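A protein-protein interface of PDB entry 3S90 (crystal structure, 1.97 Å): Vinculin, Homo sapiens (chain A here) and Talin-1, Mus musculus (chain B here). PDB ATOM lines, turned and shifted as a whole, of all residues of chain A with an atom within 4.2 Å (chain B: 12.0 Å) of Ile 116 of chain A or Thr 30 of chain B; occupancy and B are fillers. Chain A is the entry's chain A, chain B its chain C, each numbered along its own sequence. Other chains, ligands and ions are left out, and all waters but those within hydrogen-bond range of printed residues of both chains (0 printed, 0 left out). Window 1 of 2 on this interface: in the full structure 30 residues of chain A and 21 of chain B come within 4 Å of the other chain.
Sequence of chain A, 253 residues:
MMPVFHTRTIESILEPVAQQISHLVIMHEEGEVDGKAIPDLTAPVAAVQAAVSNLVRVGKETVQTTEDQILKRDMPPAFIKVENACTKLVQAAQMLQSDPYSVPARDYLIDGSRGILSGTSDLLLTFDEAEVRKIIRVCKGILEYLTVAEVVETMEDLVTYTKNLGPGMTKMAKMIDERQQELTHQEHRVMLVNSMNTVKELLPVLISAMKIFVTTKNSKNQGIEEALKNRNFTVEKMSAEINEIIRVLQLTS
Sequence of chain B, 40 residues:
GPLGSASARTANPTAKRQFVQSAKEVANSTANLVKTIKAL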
ATOM      1  N   VAL A  17     -17.370  15.943  -4.468  1.00  0.00           N
ATOM      2  CA  VAL A  17     -17.909  17.300  -4.284  1.00  0.00           C
ATOM      3  C   VAL A  17     -17.322  18.252  -5.365  1.00  0.00           C
ATOM      4  O   VAL A  17     -18.071  19.090  -5.880  1.00  0.00           O
ATOM      5  CB  VAL A  17     -17.788  17.867  -2.835  1.00  0.00           C
ATOM      6  CG1 VAL A  17     -16.341  18.080  -2.405  1.00  0.00           C
ATOM      7  CG2 VAL A  17     -18.615  19.155  -2.665  1.00  0.00           C
ATOM      8  N   VAL A  48     -24.472  22.904   6.165  1.00  0.00           N
ATOM      9  CA  VAL A  48     -23.132  23.285   5.690  1.00  0.00           C
ATOM     10  C   VAL A  48     -22.481  24.212   6.738  1.00  0.00           C
ATOM     11  O   VAL A  48     -21.323  23.990   7.089  1.00  0.00           O
ATOM     12  CB  VAL A  48     -23.149  23.927   4.273  1.00  0.00           C
ATOM     13  CG1 VAL A  48     -21.762  24.450   3.879  1.00  0.00           C
ATOM     14  CG2 VAL A  48     -23.640  22.933   3.236  1.00  0.00           C
ATOM     15  N   VAL A  52     -19.017  23.525   8.652  1.00  0.00           N
ATOM     16  CA  VAL A  52     -17.910  24.483   8.513  1.00  0.00           C
ATOM     17  C   VAL A  52     -17.447  24.952   9.919  1.00  0.00           C
ATOM     18  O   VAL A  52     -16.241  24.971  10.168  1.00  0.00           O
ATOM     19  CB  VAL A  52     -18.267  25.661   7.557  1.00  0.00           C
ATOM     20  CG1 VAL A  52     -17.315  26.850   7.722  1.00  0.00           C
ATOM     21  CG2 VAL A  52     -18.270  25.185   6.105  1.00  0.00           C
ATOM     22  N   VAL A  82     -13.460  29.577   4.069  1.00  0.00           N
ATOM     23  CA  VAL A  82     -14.644  28.710   4.222  1.00  0.00           C
ATOM     24  C   VAL A  82     -15.768  29.443   4.939  1.00  0.00           C
ATOM     25  O   VAL A  82     -16.930  29.212   4.620  1.00  0.00           O
ATOM     26  CB  VAL A  82     -14.375  27.328   4.890  1.00  0.00           C
ATOM     27  CG1 VAL A  82     -13.502  26.456   4.006  1.00  0.00           C
ATOM     28  CG2 VAL A  82     -13.758  27.464   6.279  1.00  0.00           C
ATOM     29  N   ALA A  85     -17.307  31.984   2.528  1.00  0.00           N
ATOM     30  CA  ALA A  85     -18.081  31.212   1.565  1.00  0.00           C
ATOM     31  C   ALA A  85     -19.423  30.826   2.183  1.00  0.00           C
ATOM     32  O   ALA A  85     -20.455  31.001   1.549  1.00  0.00           O
ATOM     33  CB  ALA A  85     -17.308  29.984   1.132  1.00  0.00           C
ATOM     34  N   CYS A  86     -19.404  30.388   3.446  1.00  0.00           N
ATOM     35  CA  CYS A  86     -20.591  30.036   4.225  1.00  0.00           C
ATOM     36  C   CYS A  86     -21.559  31.214   4.338  1.00  0.00           C
ATOM     37  O   CYS A  86     -22.778  31.016   4.263  1.00  0.00           O
ATOM     38  CB  CYS A  86     -20.175  29.555   5.607  1.00  0.00           C
ATOM     39  SG  CYS A  86     -20.810  27.928   6.018  1.00  0.00           S
ATOM     40  N   LEU A  89     -23.596  31.553   1.194  1.00  0.00           N
ATOM     41  CA  LEU A  89     -24.615  30.503   1.114  1.00  0.00           C
ATOM     42  C   LEU A  89     -25.809  30.803   2.037  1.00  0.00           C
ATOM     43  O   LEU A  89     -26.945  30.673   1.600  1.00  0.00           O
ATOM     44  CB  LEU A  89     -24.020  29.117   1.417  1.00  0.00           C
ATOM     45  CG  LEU A  89     -22.973  28.597   0.426  1.00  0.00           C
ATOM     46  CD1 LEU A  89     -22.347  27.299   0.921  1.00  0.00           C
ATOM     47  CD2 LEU A  89     -23.563  28.414  -0.969  1.00  0.00           C
ATOM     48  N   GLY A 112     -20.159  30.658  -3.211  1.00  0.00           N
ATOM     49  CA  GLY A 112     -20.145  30.037  -1.890  1.00  0.00           C
ATOM     50  C   GLY A 112     -19.682  28.589  -1.924  1.00  0.00           C
ATOM     51  O   GLY A 112     -18.773  28.223  -1.187  1.00  0.00           O
ATOM     52  N   SER A 113     -20.277  27.759  -2.797  1.00  0.00           N
ATOM     53  CA  SER A 113     -19.910  26.344  -2.968  1.00  0.00           C
ATOM     54  C   SER A 113     -18.446  26.199  -3.392  1.00  0.00           C
ATOM     55  O   SER A 113     -17.728  25.372  -2.830  1.00  0.00           O
ATOM     56  CB  SER A 113     -20.823  25.678  -3.996  1.00  0.00           C
ATOM     57  OG  SER A 113     -22.172  25.723  -3.560  1.00  0.00           O
ATOM     58  N   ARG A 114     -17.994  27.034  -4.353  1.00  0.00           N
ATOM     59  CA  ARG A 114     -16.605  27.061  -4.832  1.00  0.00           C
ATOM     60  C   ARG A 114     -15.651  27.446  -3.719  1.00  0.00           C
ATOM     61  O   ARG A 114     -14.584  26.851  -3.611  1.00  0.00           O
ATOM     62  CB  ARG A 114     -16.438  28.074  -5.976  1.00  0.00           C
ATOM     63  CG  ARG A 114     -16.874  27.577  -7.341  1.00  0.00           C
ATOM     64  CD  ARG A 114     -16.941  28.774  -8.277  1.00  0.00           C
ATOM     65  NE  ARG A 114     -16.166  28.557  -9.496  1.00  0.00           N
ATOM     66  CZ  ARG A 114     -16.338  29.232 -10.630  1.00  0.00           C
ATOM     67  NH1 ARG A 114     -17.253  30.190 -10.710  1.00  0.00           N
ATOM     68  NH2 ARG A 114     -15.598  28.950 -11.694  1.00  0.00           N
ATOM     69  N   GLY A 115     -16.041  28.438  -2.912  1.00  0.00           N
ATOM     70  CA  GLY A 115     -15.242  28.922  -1.797  1.00  0.00           C
ATOM     71  C   GLY A 115     -15.086  27.866  -0.722  1.00  0.00           C
ATOM     72  O   GLY A 115     -14.000  27.723  -0.170  1.00  0.00           O
ATOM     73  N   ILE A 116     -16.167  27.118  -0.426  1.00  0.00           N
ATOM     74  CA  ILE A 116     -16.169  26.020   0.545  1.00  0.00           C
ATOM     75  C   ILE A 116     -15.166  24.960   0.065  1.00  0.00           C
ATOM     76  O   ILE A 116     -14.318  24.542   0.845  1.00  0.00           O
ATOM     77  CB  ILE A 116     -17.601  25.414   0.748  1.00  0.00           C
ATOM     78  CG1 ILE A 116     -18.600  26.386   1.447  1.00  0.00           C
ATOM     79  CG2 ILE A 116     -17.545  24.037   1.437  1.00  0.00           C
ATOM     80  CD1 ILE A 116     -18.319  26.741   2.829  1.00  0.00           C
ATOM     81  N   LEU A 117     -15.244  24.563  -1.217  1.00  0.00           N
ATOM     82  CA  LEU A 117     -14.330  23.577  -1.805  1.00  0.00           C
ATOM     83  C   LEU A 117     -12.870  24.041  -1.755  1.00  0.00           C
ATOM     84  O   LEU A 117     -12.017  23.290  -1.292  1.00  0.00           O
ATOM     85  CB  LEU A 117     -14.717  23.237  -3.259  1.00  0.00           C
ATOM     86  CG  LEU A 117     -13.778  22.238  -3.991  1.00  0.00           C
ATOM     87  CD1 LEU A 117     -13.800  20.825  -3.356  1.00  0.00           C
ATOM     88  CD2 LEU A 117     -14.098  22.175  -5.452  1.00  0.00           C
ATOM     89  N   SER A 118     -12.589  25.254  -2.251  1.00  0.00           N
ATOM     90  CA  SER A 118     -11.254  25.844  -2.294  1.00  0.00           C
ATOM     91  C   SER A 118     -10.621  25.937  -0.875  1.00  0.00           C
ATOM     92  O   SER A 118      -9.471  25.534  -0.704  1.00  0.00           O
ATOM     93  CB  SER A 118     -11.311  27.216  -2.959  1.00  0.00           C
ATOM     94  OG  SER A 118     -10.057  27.877  -2.932  1.00  0.00           O
ATOM     95  N   GLY A 119     -11.387  26.410   0.113  1.00  0.00           N
ATOM     96  CA  GLY A 119     -10.926  26.507   1.491  1.00  0.00           C
ATOM     97  C   GLY A 119     -10.691  25.151   2.129  1.00  0.00           C
ATOM     98  O   GLY A 119      -9.682  24.962   2.798  1.00  0.00           O
ATOM     99  N   THR A 120     -11.612  24.186   1.910  1.00  0.00           N
ATOM    100  CA  THR A 120     -11.485  22.834   2.454  1.00  0.00           C
ATOM    101  C   THR A 120     -10.253  22.152   1.820  1.00  0.00           C
ATOM    102  O   THR A 120      -9.495  21.508   2.530  1.00  0.00           O
ATOM    103  CB  THR A 120     -12.774  22.031   2.260  1.00  0.00           C
ATOM    104  OG1 THR A 120     -13.836  22.767   2.843  1.00  0.00           O
ATOM    105  CG2 THR A 120     -12.711  20.631   2.929  1.00  0.00           C
ATOM    106  N   PHE B  19      -9.855  15.905  12.512  1.00  0.00           N
ATOM    107  CA  PHE B  19      -9.700  16.919  11.466  1.00  0.00           C
ATOM    108  C   PHE B  19     -10.232  16.412  10.131  1.00  0.00           C
ATOM    109  O   PHE B  19     -10.999  17.123   9.476  1.00  0.00           O
ATOM    110  CB  PHE B  19      -8.228  17.356  11.327  1.00  0.00           C
ATOM    111  CG  PHE B  19      -8.005  18.401  10.255  1.00  0.00           C
ATOM    112  CD1 PHE B  19      -8.198  19.750  10.526  1.00  0.00           C
ATOM    113  CD2 PHE B  19      -7.638  18.030   8.966  1.00  0.00           C
ATOM    114  CE1 PHE B  19      -8.021  20.711   9.527  1.00  0.00           C
ATOM    115  CE2 PHE B  19      -7.469  18.991   7.967  1.00  0.00           C
ATOM    116  CZ  PHE B  19      -7.658  20.324   8.254  1.00  0.00           C
ATOM    117  N   GLN B  21     -12.292  13.797   9.559  1.00  0.00           N
ATOM    118  CA  GLN B  21     -13.740  13.558   9.697  1.00  0.00           C
ATOM    119  C   GLN B  21     -14.535  14.874   9.564  1.00  0.00           C
ATOM    120  O   GLN B  21     -15.613  14.871   8.965  1.00  0.00           O
ATOM    121  CB  GLN B  21     -14.063  12.857  11.037  1.00  0.00           C
ATOM    122  CG  GLN B  21     -15.518  12.364  11.192  1.00  0.00           C
ATOM    123  CD  GLN B  21     -16.011  11.505  10.045  1.00  0.00           C
ATOM    124  OE1 GLN B  21     -15.429  10.466   9.711  1.00  0.00           O
ATOM    125  NE2 GLN B  21     -17.100  11.928   9.413  1.00  0.00           N
ATOM    126  N   SER B  22     -13.994  15.984  10.111  1.00  0.00           N
ATOM    127  CA  SER B  22     -14.590  17.319  10.026  1.00  0.00           C
ATOM    128  C   SER B  22     -14.633  17.802   8.571  1.00  0.00           C
ATOM    129  O   SER B  22     -15.665  18.318   8.144  1.00  0.00           O
ATOM    130  CB  SER B  22     -13.821  18.312  10.889  1.00  0.00           C
ATOM    131  OG  SER B  22     -14.112  18.081  12.255  1.00  0.00           O
ATOM    132  N   ALA B  23     -13.526  17.608   7.812  1.00  0.00           N
ATOM    133  CA  ALA B  23     -13.414  17.980   6.400  1.00  0.00           C
ATOM    134  C   ALA B  23     -14.386  17.166   5.567  1.00  0.00           C
ATOM    135  O   ALA B  23     -15.073  17.730   4.713  1.00  0.00           O
ATOM    136  CB  ALA B  23     -11.996  17.773   5.905  1.00  0.00           C
ATOM    137  N   LYS B  24     -14.475  15.844   5.847  1.00  0.00           N
ATOM    138  CA  LYS B  24     -15.393  14.919   5.180  1.00  0.00           C
ATOM    139  C   LYS B  24     -16.843  15.394   5.350  1.00  0.00           C
ATOM    140  O   LYS B  24     -17.594  15.373   4.380  1.00  0.00           O
ATOM    141  CB  LYS B  24     -15.220  13.500   5.744  1.00  0.00           C
ATOM    142  CG  LYS B  24     -15.356  12.407   4.703  1.00  0.00           C
ATOM    143  CD  LYS B  24     -15.081  11.033   5.312  1.00  0.00           C
ATOM    144  CE  LYS B  24     -14.975   9.931   4.279  1.00  0.00           C
ATOM    145  NZ  LYS B  24     -16.296   9.574   3.697  1.00  0.00           N
ATOM    146  N   GLU B  25     -17.205  15.880   6.561  1.00  0.00           N
ATOM    147  CA  GLU B  25     -18.542  16.383   6.887  1.00  0.00           C
ATOM    148  C   GLU B  25     -18.900  17.635   6.067  1.00  0.00           C
ATOM    149  O   GLU B  25     -20.040  17.760   5.612  1.00  0.00           O
ATOM    150  CB  GLU B  25     -18.661  16.682   8.387  1.00  0.00           C
ATOM    151  CG  GLU B  25     -20.025  16.331   8.957  1.00  0.00           C
ATOM    152  CD  GLU B  25     -20.258  14.843   9.150  1.00  0.00           C
ATOM    153  OE1 GLU B  25     -19.876  14.317  10.219  1.00  0.00           O
ATOM    154  OE2 GLU B  25     -20.796  14.197   8.220  1.00  0.00           O
ATOM    155  N   VAL B  26     -17.914  18.541   5.869  1.00  0.00           N
ATOM    156  CA  VAL B  26     -18.053  19.759   5.070  1.00  0.00           C
ATOM    157  C   VAL B  26     -18.298  19.358   3.611  1.00  0.00           C
ATOM    158  O   VAL B  26     -19.226  19.875   2.997  1.00  0.00           O
ATOM    159  CB  VAL B  26     -16.831  20.708   5.227  1.00  0.00           C
ATOM    160  CG1 VAL B  26     -16.854  21.836   4.198  1.00  0.00           C
ATOM    161  CG2 VAL B  26     -16.778  21.289   6.625  1.00  0.00           C
ATOM    162  N   ALA B  27     -17.489  18.416   3.075  1.00  0.00           N
ATOM    163  CA  ALA B  27     -17.615  17.935   1.696  1.00  0.00           C
ATOM    164  C   ALA B  27     -18.986  17.301   1.457  1.00  0.00           C
ATOM    165  O   ALA B  27     -19.633  17.630   0.466  1.00  0.00           O
ATOM    166  CB  ALA B  27     -16.507  16.932   1.383  1.00  0.00           C
ATOM    167  N   ASN B  28     -19.435  16.423   2.385  1.00  0.00           N
ATOM    168  CA  ASN B  28     -20.713  15.708   2.337  1.00  0.00           C
ATOM    169  C   ASN B  28     -21.915  16.658   2.357  1.00  0.00           C
ATOM    170  O   ASN B  28     -22.827  16.494   1.545  1.00  0.00           O
ATOM    171  CB  ASN B  28     -20.820  14.705   3.502  1.00  0.00           C
ATOM    172  CG  ASN B  28     -19.939  13.480   3.379  1.00  0.00           C
ATOM    173  OD1 ASN B  28     -19.399  13.155   2.311  1.00  0.00           O
ATOM    174  ND2 ASN B  28     -19.781  12.760   4.485  1.00  0.00           N
ATOM    175  N   SER B  29     -21.918  17.642   3.274  1.00  0.00           N
ATOM    176  CA  SER B  29     -23.005  18.617   3.385  1.00  0.00           C
ATOM    177  C   SER B  29     -23.052  19.533   2.151  1.00  0.00           C
ATOM    178  O   SER B  29     -24.147  19.849   1.679  1.00  0.00           O
ATOM    179  CB  SER B  29     -22.866  19.434   4.665  1.00  0.00           C
ATOM    180  OG  SER B  29     -21.654  20.171   4.671  1.00  0.00           O
ATOM    181  N   THR B  30     -21.878  19.938   1.621  1.00  0.00           N
ATOM    182  CA  THR B  30     -21.785  20.783   0.425  1.00  0.00           C
ATOM    183  C   THR B  30     -22.277  19.985  -0.775  1.00  0.00           C
ATOM    184  O   THR B  30     -23.064  20.513  -1.553  1.00  0.00           O
ATOM    185  CB  THR B  30     -20.371  21.339   0.237  1.00  0.00           C
ATOM    186  OG1 THR B  30     -20.023  22.025   1.433  1.00  0.00           O
ATOM    187  CG2 THR B  30     -20.266  22.323  -0.924  1.00  0.00           C
ATOM    188  N   ALA B  31     -21.876  18.699  -0.888  1.00  0.00           N
ATOM    189  CA  ALA B  31     -22.334  17.822  -1.971  1.00  0.00           C
ATOM    190  C   ALA B  31     -23.867  17.747  -1.997  1.00  0.00           C
ATOM    191  O   ALA B  31     -24.456  17.923  -3.063  1.00  0.00           O
ATOM    192  CB  ALA B  31     -21.738  16.429  -1.817  1.00  0.00           C
ATOM    193  N   ASN B  32     -24.505  17.550  -0.818  1.00  0.00           N
ATOM    194  CA  ASN B  32     -25.962  17.465  -0.643  1.00  0.00           C
ATOM    195  C   ASN B  32     -26.628  18.785  -1.024  1.00  0.00           C
ATOM    196  O   ASN B  32     -27.710  18.765  -1.612  1.00  0.00           O
ATOM    197  CB  ASN B  32     -26.306  17.064   0.805  1.00  0.00           C
ATOM    198  CG  ASN B  32     -27.777  17.116   1.164  1.00  0.00           C
ATOM    199  OD1 ASN B  32     -28.633  16.484   0.530  1.00  0.00           O
ATOM    200  ND2 ASN B  32     -28.099  17.856   2.215  1.00  0.00           N
ATOM    201  N   LEU B  33     -25.976  19.929  -0.723  1.00  0.00           N
ATOM    202  CA  LEU B  33     -26.497  21.241  -1.092  1.00  0.00           C
ATOM    203  C   LEU B  33     -26.433  21.443  -2.617  1.00  0.00           C
ATOM    204  O   LEU B  33     -27.416  21.888  -3.200  1.00  0.00           O
ATOM    205  CB  LEU B  33     -25.725  22.361  -0.364  1.00  0.00           C
ATOM    206  CG  LEU B  33     -26.037  23.815  -0.767  1.00  0.00           C
ATOM    207  CD1 LEU B  33     -27.508  24.194  -0.498  1.00  0.00           C
ATOM    208  CD2 LEU B  33     -25.077  24.774  -0.111  1.00  0.00           C
ATOM    209  N   VAL B  34     -25.286  21.117  -3.250  1.00  0.00           N
ATOM    210  CA  VAL B  34     -25.055  21.290  -4.692  1.00  0.00           C
ATOM    211  C   VAL B  34     -26.031  20.401  -5.479  1.00  0.00           C
ATOM    212  O   VAL B  34     -26.589  20.857  -6.475  1.00  0.00           O
ATOM    213  CB  VAL B  34     -23.570  21.045  -5.080  1.00  0.00           C
ATOM    214  CG1 VAL B  34     -23.361  21.095  -6.589  1.00  0.00           C
ATOM    215  CG2 VAL B  34     -22.667  22.076  -4.412  1.00  0.00           C
ATOM    216  N   LYS B  35     -26.276  19.164  -4.992  1.00  0.00           N
ATOM    217  CA  LYS B  35     -27.209  18.196  -5.573  1.00  0.00           C
ATOM    218  C   LYS B  35     -28.641  18.762  -5.508  1.00  0.00           C
ATOM    219  O   LYS B  35     -29.382  18.629  -6.487  1.00  0.00           O
ATOM    220  CB  LYS B  35     -27.084  16.844  -4.835  1.00  0.00           C
ATOM    221  CG  LYS B  35     -27.958  15.715  -5.383  1.00  0.00           C
ATOM    222  CD  LYS B  35     -27.629  14.361  -4.745  1.00  0.00           C
ATOM    223  CE  LYS B  35     -28.394  14.057  -3.469  1.00  0.00           C
ATOM    224  NZ  LYS B  35     -29.809  13.669  -3.736  1.00  0.00           N
ATOM    225  N   THR B  36     -29.005  19.431  -4.384  1.00  0.00           N
ATOM    226  CA  THR B  36     -30.323  20.066  -4.191  1.00  0.00           C
ATOM    227  C   THR B  36     -30.487  21.266  -5.155  1.00  0.00           C
ATOM    228  O   THR B  36     -31.572  21.430  -5.707  1.00  0.00           O
ATOM    229  CB  THR B  36     -30.539  20.468  -2.712  1.00  0.00           C
ATOM    230  OG1 THR B  36     -30.324  19.328  -1.883  1.00  0.00           O
ATOM    231  CG2 THR B  36     -31.949  21.004  -2.440  1.00  0.00           C
ATOM    232  N   ILE B  37     -29.425  22.085  -5.365  1.00  0.00           N
ATOM    233  CA  ILE B  37     -29.469  23.239  -6.281  1.00  0.00           C
ATOM    234  C   ILE B  37     -29.611  22.753  -7.736  1.00  0.00           C
ATOM    235  O   ILE B  37     -30.481  23.233  -8.451  1.00  0.00           O
ATOM    236  CB  ILE B  37     -28.237  24.177  -6.133  1.00  0.00           C
ATOM    237  CG1 ILE B  37     -28.120  24.746  -4.699  1.00  0.00           C
ATOM    238  CG2 ILE B  37     -28.284  25.320  -7.180  1.00  0.00           C
ATOM    239  CD1 ILE B  37     -26.704  25.171  -4.296  1.00  0.00           C
ATOM    240  N   LYS B  38     -28.742  21.810  -8.147  1.00  0.00           N
ATOM    241  CA  LYS B  38     -28.636  21.212  -9.481  1.00  0.00           C
ATOM    242  C   LYS B  38     -29.900  20.450  -9.910  1.00  0.00           C
ATOM    243  O   LYS B  38     -30.172  20.376 -11.109  1.00  0.00           O
ATOM    244  CB  LYS B  38     -27.444  20.240  -9.495  1.00  0.00           C
ATOM    245  CG  LYS B  38     -26.904  19.900 -10.873  1.00  0.00           C
ATOM    246  CD  LYS B  38     -26.070  18.638 -10.880  1.00  0.00           C
ATOM    247  CE  LYS B  38     -24.627  18.963 -10.617  1.00  0.00           C
ATOM    248  NZ  LYS B  38     -24.299  18.918  -9.176  1.00  0.00           N
ATOM    249  N   ALA B  39     -30.626  19.840  -8.937  1.00  0.00           N
ATOM    250  CA  ALA B  39     -31.828  19.002  -9.112  1.00  0.00           C
ATOM    251  C   ALA B  39     -32.738  19.479 -10.240  1.00  0.00           C
ATOM    252  O   ALA B  39     -33.125  20.649 -10.281  1.00  0.00           O
ATOM    253  CB  ALA B  39     -32.615  18.928  -7.810  1.00  0.00           C
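Among the printed residues, merely in contact across the chains: Ile 116 of chain A with Thr 30 of chain B, Thr 120 of chain A with Val 26 of chain B, Val 48 of chain A with Ser 29 of chain B, Ile 116 of chain A with Val 26 of chain B, Val 17 of chain A with Ala 27 of chain B, Val 17 of chain A with Ala 31 of chain B, Val 52 of chain A with Val 26 of chain B, Ser 113 of chain A with Val 34 of chain B, Val 48 of chain A with Thr 30 of chain B, Leu 89 of chain A with Leu 33 of chain B and Val 17 of chain A with Thr 30 of chain B.
Of the 16 printed residues of chain A, 7 touch a printed residue of chain B. Of the 20 printed residues of chain B, 7 touch a printed residue of chain A.
Val 17 of chain A touches just these residues of chain B: Ala 27, Thr 30 and Ala 31. Val 48 of chain A touches two residues of chain B. Of chain B, only Val 26 comes within 4 Å of Val 52 of chain A. No residue of chain B comes within 4 Å of Val 82 of chain A. No residue of chain B comes within 4 Å of Ala 85 of chain A. Printed residues of chain B within 4 Å of Leu 89 of chain A: Leu 33. Ser 113 of chain A touches just one residue of chain B: Val 34. Of chain B, only Val 26 and Thr 30 come within 4 Å of Ile 116 of chain A. No residue of chain B comes within 4 Å of Leu 117 of chain A. No residue of chain B comes within 4 Å of Ser 118 of chain A. No residue of chain B comes within 4 Å of Gly 119 of chain A. Thr 120 of chain A touches one residue of chain B. Of the printed residues of chain A, Ser 29 of chain B touches Val 48 (3.5 Å). Of chain A, only Val 17 (3.97 Å), Val 48 (3.8 Å) and Ile 116 (3.2 Å) come within 4 Å of Thr 30 of chain B. Asn 32 of chain B touches none of the printed residues of chain A. Of the printed residues of chain A, Leu 33 of chain B touches Leu 89 (3.9 Å). Printed residues of chain A within 4 Å of Val 34 of chain B: Ser 113.
OG1 of Thr 120 of chain A lies within hydrogen-bond range of O of Ile 116 of chain A (2.7 Å). The backbone carbonyl oxygen (O) of Glu 25 of chain B sits at hydrogen-bond distance from the side-chain hydroxyl (OG) of Ser 29 of chain B (3.1 Å). The side-chain hydroxyl (OG) of Ser 29 of chain B sits at hydrogen-bond distance from the backbone carbonyl oxygen (O) of Val 26 of chain B (3.0 Å). O of Val 26 of chain B sits at hydrogen-bond distance from OG1 of Thr 30 of chain B, at 2.8 Å.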
